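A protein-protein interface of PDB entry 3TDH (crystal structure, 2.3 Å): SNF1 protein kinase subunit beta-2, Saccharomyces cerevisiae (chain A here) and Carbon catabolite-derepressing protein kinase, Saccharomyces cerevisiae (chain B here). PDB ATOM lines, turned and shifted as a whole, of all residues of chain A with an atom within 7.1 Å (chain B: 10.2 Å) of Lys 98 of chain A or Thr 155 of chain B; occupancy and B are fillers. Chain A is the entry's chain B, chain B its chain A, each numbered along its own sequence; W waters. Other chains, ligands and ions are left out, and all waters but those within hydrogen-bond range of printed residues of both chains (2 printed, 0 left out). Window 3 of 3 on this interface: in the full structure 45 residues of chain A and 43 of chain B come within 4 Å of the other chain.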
ATOM      1  N   VAL A  95     -27.592  16.630 -15.344  1.00  0.00           N
ATOM      2  CA  VAL A  95     -27.628  15.306 -15.960  1.00  0.00           C
ATOM      3  C   VAL A  95     -28.512  14.311 -15.188  1.00  0.00           C
ATOM      4  O   VAL A  95     -28.805  14.493 -13.994  1.00  0.00           O
ATOM      5  CB  VAL A  95     -26.204  14.709 -16.139  1.00  0.00           C
ATOM      6  CG1 VAL A  95     -25.297  15.668 -16.922  1.00  0.00           C
ATOM      7  CG2 VAL A  95     -25.583  14.369 -14.794  1.00  0.00           C
ATOM      8  N   ARG A  96     -28.912  13.250 -15.879  1.00  0.00           N
ATOM      9  CA  ARG A  96     -29.707  12.194 -15.277  1.00  0.00           C
ATOM     10  C   ARG A  96     -28.817  11.124 -14.658  1.00  0.00           C
ATOM     11  O   ARG A  96     -27.866  10.657 -15.280  1.00  0.00           O
ATOM     12  CB  ARG A  96     -30.642  11.566 -16.319  1.00  0.00           C
ATOM     13  N   TYR A  97     -29.112  10.769 -13.415  1.00  0.00           N
ATOM     14  CA  TYR A  97     -28.583   9.546 -12.836  1.00  0.00           C
ATOM     15  C   TYR A  97     -29.750   8.651 -12.428  1.00  0.00           C
ATOM     16  O   TYR A  97     -30.462   8.938 -11.460  1.00  0.00           O
ATOM     17  CB  TYR A  97     -27.634   9.814 -11.658  1.00  0.00           C
ATOM     18  CG  TYR A  97     -27.045   8.536 -11.110  1.00  0.00           C
ATOM     19  CD1 TYR A  97     -26.133   7.799 -11.858  1.00  0.00           C
ATOM     20  CD2 TYR A  97     -27.419   8.049  -9.856  1.00  0.00           C
ATOM     21  CE1 TYR A  97     -25.594   6.618 -11.377  1.00  0.00           C
ATOM     22  CE2 TYR A  97     -26.881   6.855  -9.360  1.00  0.00           C
ATOM     23  CZ  TYR A  97     -25.968   6.148 -10.134  1.00  0.00           C
ATOM     24  OH  TYR A  97     -25.424   4.968  -9.678  1.00  0.00           O
ATOM     25  N   LYS A  98     -29.928   7.571 -13.184  1.00  0.00           N
ATOM     26  CA  LYS A  98     -31.108   6.701 -13.091  1.00  0.00           C
ATOM     27  C   LYS A  98     -32.382   7.535 -13.236  1.00  0.00           C
ATOM     28  O   LYS A  98     -32.614   8.110 -14.294  1.00  0.00           O
ATOM     29  CB  LYS A  98     -31.100   5.861 -11.803  1.00  0.00           C
ATOM     30  CG  LYS A  98     -29.791   5.109 -11.524  1.00  0.00           C
ATOM     31  CD  LYS A  98     -29.328   4.290 -12.725  1.00  0.00           C
ATOM     32  CE  LYS A  98     -27.888   3.825 -12.550  1.00  0.00           C
ATOM     33  NZ  LYS A  98     -27.403   3.091 -13.758  1.00  0.00           N
ATOM     34  N   GLN A  99     -33.177   7.629 -12.172  1.00  0.00           N
ATOM     35  CA  GLN A  99     -34.400   8.427 -12.188  1.00  0.00           C
ATOM     36  C   GLN A  99     -34.233   9.732 -11.418  1.00  0.00           C
ATOM     37  O   GLN A  99     -35.209  10.410 -11.099  1.00  0.00           O
ATOM     38  CB  GLN A  99     -35.584   7.623 -11.625  1.00  0.00           C
ATOM     39  CG  GLN A  99     -35.923   6.377 -12.425  1.00  0.00           C
ATOM     40  CD  GLN A  99     -36.257   6.688 -13.872  1.00  0.00           C
ATOM     41  OE1 GLN A  99     -37.200   7.420 -14.165  1.00  0.00           O
ATOM     42  NE2 GLN A  99     -35.483   6.129 -14.786  1.00  0.00           N
ATOM     43  N   LYS A 100     -32.988  10.083 -11.122  1.00  0.00           N
ATOM     44  CA  LYS A 100     -32.716  11.288 -10.355  1.00  0.00           C
ATOM     45  C   LYS A 100     -31.876  12.271 -11.165  1.00  0.00           C
ATOM     46  O   LYS A 100     -31.395  11.941 -12.249  1.00  0.00           O
ATOM     47  CB  LYS A 100     -32.093  10.929  -8.997  1.00  0.00           C
ATOM     48  CG  LYS A 100     -33.022  10.033  -8.159  1.00  0.00           C
ATOM     49  CD  LYS A 100     -32.493   9.704  -6.774  1.00  0.00           C
ATOM     50  CE  LYS A 100     -33.565   8.959  -5.979  1.00  0.00           C
ATOM     51  NZ  LYS A 100     -33.155   8.669  -4.589  1.00  0.00           N
ATOM     52  N   TYR A 101     -31.730  13.487 -10.648  1.00  0.00           N
ATOM     53  CA  TYR A 101     -31.098  14.559 -11.400  1.00  0.00           C
ATOM     54  C   TYR A 101     -29.967  15.207 -10.612  1.00  0.00           C
ATOM     55  O   TYR A 101     -30.172  15.706  -9.502  1.00  0.00           O
ATOM     56  CB  TYR A 101     -32.148  15.587 -11.838  1.00  0.00           C
ATOM     57  CG  TYR A 101     -33.284  14.969 -12.640  1.00  0.00           C
ATOM     58  CD1 TYR A 101     -33.186  14.829 -14.022  1.00  0.00           C
ATOM     59  CD2 TYR A 101     -34.440  14.500 -12.010  1.00  0.00           C
ATOM     60  CE1 TYR A 101     -34.211  14.256 -14.762  1.00  0.00           C
ATOM     61  CE2 TYR A 101     -35.478  13.920 -12.745  1.00  0.00           C
ATOM     62  CZ  TYR A 101     -35.354  13.808 -14.120  1.00  0.00           C
ATOM     63  OH  TYR A 101     -36.360  13.238 -14.863  1.00  0.00           O
ATOM     64  N   PHE B 132     -23.649  18.583 -24.595  1.00  0.00           N
ATOM     65  CA  PHE B 132     -22.900  17.330 -24.694  1.00  0.00           C
ATOM     66  C   PHE B 132     -23.708  16.332 -25.517  1.00  0.00           C
ATOM     67  O   PHE B 132     -24.915  16.191 -25.314  1.00  0.00           O
ATOM     68  CB  PHE B 132     -22.605  16.774 -23.293  1.00  0.00           C
ATOM     69  CG  PHE B 132     -21.960  15.416 -23.295  1.00  0.00           C
ATOM     70  CD1 PHE B 132     -20.599  15.275 -23.560  1.00  0.00           C
ATOM     71  CD2 PHE B 132     -22.712  14.275 -23.026  1.00  0.00           C
ATOM     72  CE1 PHE B 132     -19.998  14.018 -23.561  1.00  0.00           C
ATOM     73  CE2 PHE B 132     -22.122  13.010 -23.025  1.00  0.00           C
ATOM     74  CZ  PHE B 132     -20.761  12.882 -23.291  1.00  0.00           C
ATOM     75  N   TRP B 135     -20.071  10.163 -26.984  1.00  0.00           N
ATOM     76  CA  TRP B 135     -18.708   9.822 -27.373  1.00  0.00           C
ATOM     77  C   TRP B 135     -18.684   8.973 -28.639  1.00  0.00           C
ATOM     78  O   TRP B 135     -19.643   8.252 -28.933  1.00  0.00           O
ATOM     79  CB  TRP B 135     -18.001   9.068 -26.244  1.00  0.00           C
ATOM     80  CG  TRP B 135     -17.851   9.848 -24.969  1.00  0.00           C
ATOM     81  CD1 TRP B 135     -18.751   9.926 -23.943  1.00  0.00           C
ATOM     82  CD2 TRP B 135     -16.727  10.644 -24.579  1.00  0.00           C
ATOM     83  NE1 TRP B 135     -18.257  10.726 -22.940  1.00  0.00           N
ATOM     84  CE2 TRP B 135     -17.017  11.181 -23.305  1.00  0.00           C
ATOM     85  CE3 TRP B 135     -15.502  10.960 -25.185  1.00  0.00           C
ATOM     86  CZ2 TRP B 135     -16.127  12.016 -22.623  1.00  0.00           C
ATOM     87  CZ3 TRP B 135     -14.616  11.791 -24.505  1.00  0.00           C
ATOM     88  CH2 TRP B 135     -14.935  12.308 -23.238  1.00  0.00           C
ATOM     89  N   SER B 154     -28.134   7.853 -18.676  1.00  0.00           N
ATOM     90  CA  SER B 154     -28.654   7.448 -17.368  1.00  0.00           C
ATOM     91  C   SER B 154     -27.557   7.328 -16.310  1.00  0.00           C
ATOM     92  O   SER B 154     -27.848   7.269 -15.111  1.00  0.00           O
ATOM     93  CB  SER B 154     -29.419   6.126 -17.476  1.00  0.00           C
ATOM     94  OG  SER B 154     -30.730   6.334 -17.970  1.00  0.00           O
ATOM     95  N   THR B 155     -26.306   7.274 -16.765  1.00  0.00           N
ATOM     96  CA  THR B 155     -25.143   7.143 -15.886  1.00  0.00           C
ATOM     97  C   THR B 155     -23.904   7.681 -16.600  1.00  0.00           C
ATOM     98  O   THR B 155     -23.236   6.937 -17.327  1.00  0.00           O
ATOM     99  CB  THR B 155     -24.883   5.661 -15.483  1.00  0.00           C
ATOM    100  OG1 THR B 155     -26.121   4.998 -15.184  1.00  0.00           O
ATOM    101  CG2 THR B 155     -23.957   5.579 -14.274  1.00  0.00           C
ATOM    102  N   PHE B 156     -23.600   8.966 -16.406  1.00  0.00           N
ATOM    103  CA  PHE B 156     -22.410   9.555 -17.034  1.00  0.00           C
ATOM    104  C   PHE B 156     -21.898  10.846 -16.388  1.00  0.00           C
ATOM    105  O   PHE B 156     -22.627  11.538 -15.675  1.00  0.00           O
ATOM    106  CB  PHE B 156     -22.631   9.767 -18.537  1.00  0.00           C
ATOM    107  CG  PHE B 156     -23.382  11.015 -18.869  1.00  0.00           C
ATOM    108  CD1 PHE B 156     -22.702  12.155 -19.282  1.00  0.00           C
ATOM    109  CD2 PHE B 156     -24.769  11.056 -18.774  1.00  0.00           C
ATOM    110  CE1 PHE B 156     -23.387  13.315 -19.588  1.00  0.00           C
ATOM    111  CE2 PHE B 156     -25.466  12.215 -19.082  1.00  0.00           C
ATOM    112  CZ  PHE B 156     -24.771  13.343 -19.490  1.00  0.00           C
ATOM    113  N   SER B 157     -20.635  11.155 -16.667  1.00  0.00           N
ATOM    114  CA  SER B 157     -19.977  12.343 -16.143  1.00  0.00           C
ATOM    115  C   SER B 157     -19.900  13.447 -17.195  1.00  0.00           C
ATOM    116  O   SER B 157     -19.443  13.220 -18.317  1.00  0.00           O
ATOM    117  CB  SER B 157     -18.571  11.997 -15.654  1.00  0.00           C
ATOM    118  OG  SER B 157     -17.890  13.151 -15.197  1.00  0.00           O
ATOM    119  N   ALA B 158     -20.345  14.641 -16.810  1.00  0.00           N
ATOM    120  CA  ALA B 158     -20.263  15.810 -17.673  1.00  0.00           C
ATOM    121  C   ALA B 158     -18.941  16.552 -17.508  1.00  0.00           C
ATOM    122  O   ALA B 158     -18.681  17.515 -18.222  1.00  0.00           O
ATOM    123  CB  ALA B 158     -21.427  16.751 -17.401  1.00  0.00           C
HETATM  124  O   HOH W   1     -25.129  10.551 -14.602  1.00  0.00           O
HETATM  125  O   HOH W   2     -32.607   7.939 -16.859  1.00  0.00           O
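O of Ser 154 of chain B is in hydrogen-bond range of N of Lys 98 of chain A (2.9 Å). O of Arg 96 of chain A lies close to O of Ser 154 of chain B (3.4 Å). OG1 of Thr 155 of chain B lies within hydrogen-bond range of NZ of Lys 98 of chain A, at 2.7 Å.
Hydrophobic or aromatic side chains of chain A within 4 Å of the printed part of chain B: Val 95 and Tyr 97. Along chain A the printed residues that touch a printed residue of chain B span positions 95 to 98. Among the printed residues, 6 pairs touch across the chains.
Water W2 bridges O of Lys 98 of chain A (2.6 Å) and OG of Ser 154 of chain B (2.7 Å). Water W1 lies within hydrogen-bond range of O of Arg 96 of chain A (2.8 Å) and N of Phe 156 of chain B (2.8 Å).
Lys 98 of chain A touches just these residues of chain B: Ser 154 (2.9 Å) and Thr 155 (2.7 Å). Of the printed residues of chain A, Thr 155 of chain B touches Tyr 97 (3.5 Å) and Lys 98 (2.7 Å). Tyr 97 of chain A touches just these residues of chain B: Ser 154 and Thr 155. No residue of chain B comes within 4 Å of Gln 99 of chain A. Printed residues of chain A within 4 Å of Phe 156 of chain B: Val 95 (3.5 Å). Printed residues of chain B within 4 Å of Arg 96 of chain A: Ser 154 (3.4 Å). Of the printed residues of chain B, Val 95 of chain A touches Phe 156 (3.5 Å). Printed residues of chain A within 4 Å of Ser 154 of chain B: Arg 96, Tyr 97 and Lys 98. The nearest residue of chain B that does not touch Lys 98 of chain A is Phe 156 of chain B (7.2 Å). The nearest printed residue of chain A that does not touch Thr 155 of chain B is Arg 96 of chain A (4.01 Å). The nearest printed residue of chain A that does not touch Phe 156 of chain B is Arg 96 of chain A (4.7 Å).
Among the printed residues, pairs that only touch across the chains: Val 95 of chain A with Phe 156 of chain B (3.5 Å), Tyr 97 of chain A with Ser 154 of chain B (3.3 Å) and Tyr 97 of chain A with Thr 155 of chain B (3.5 Å).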
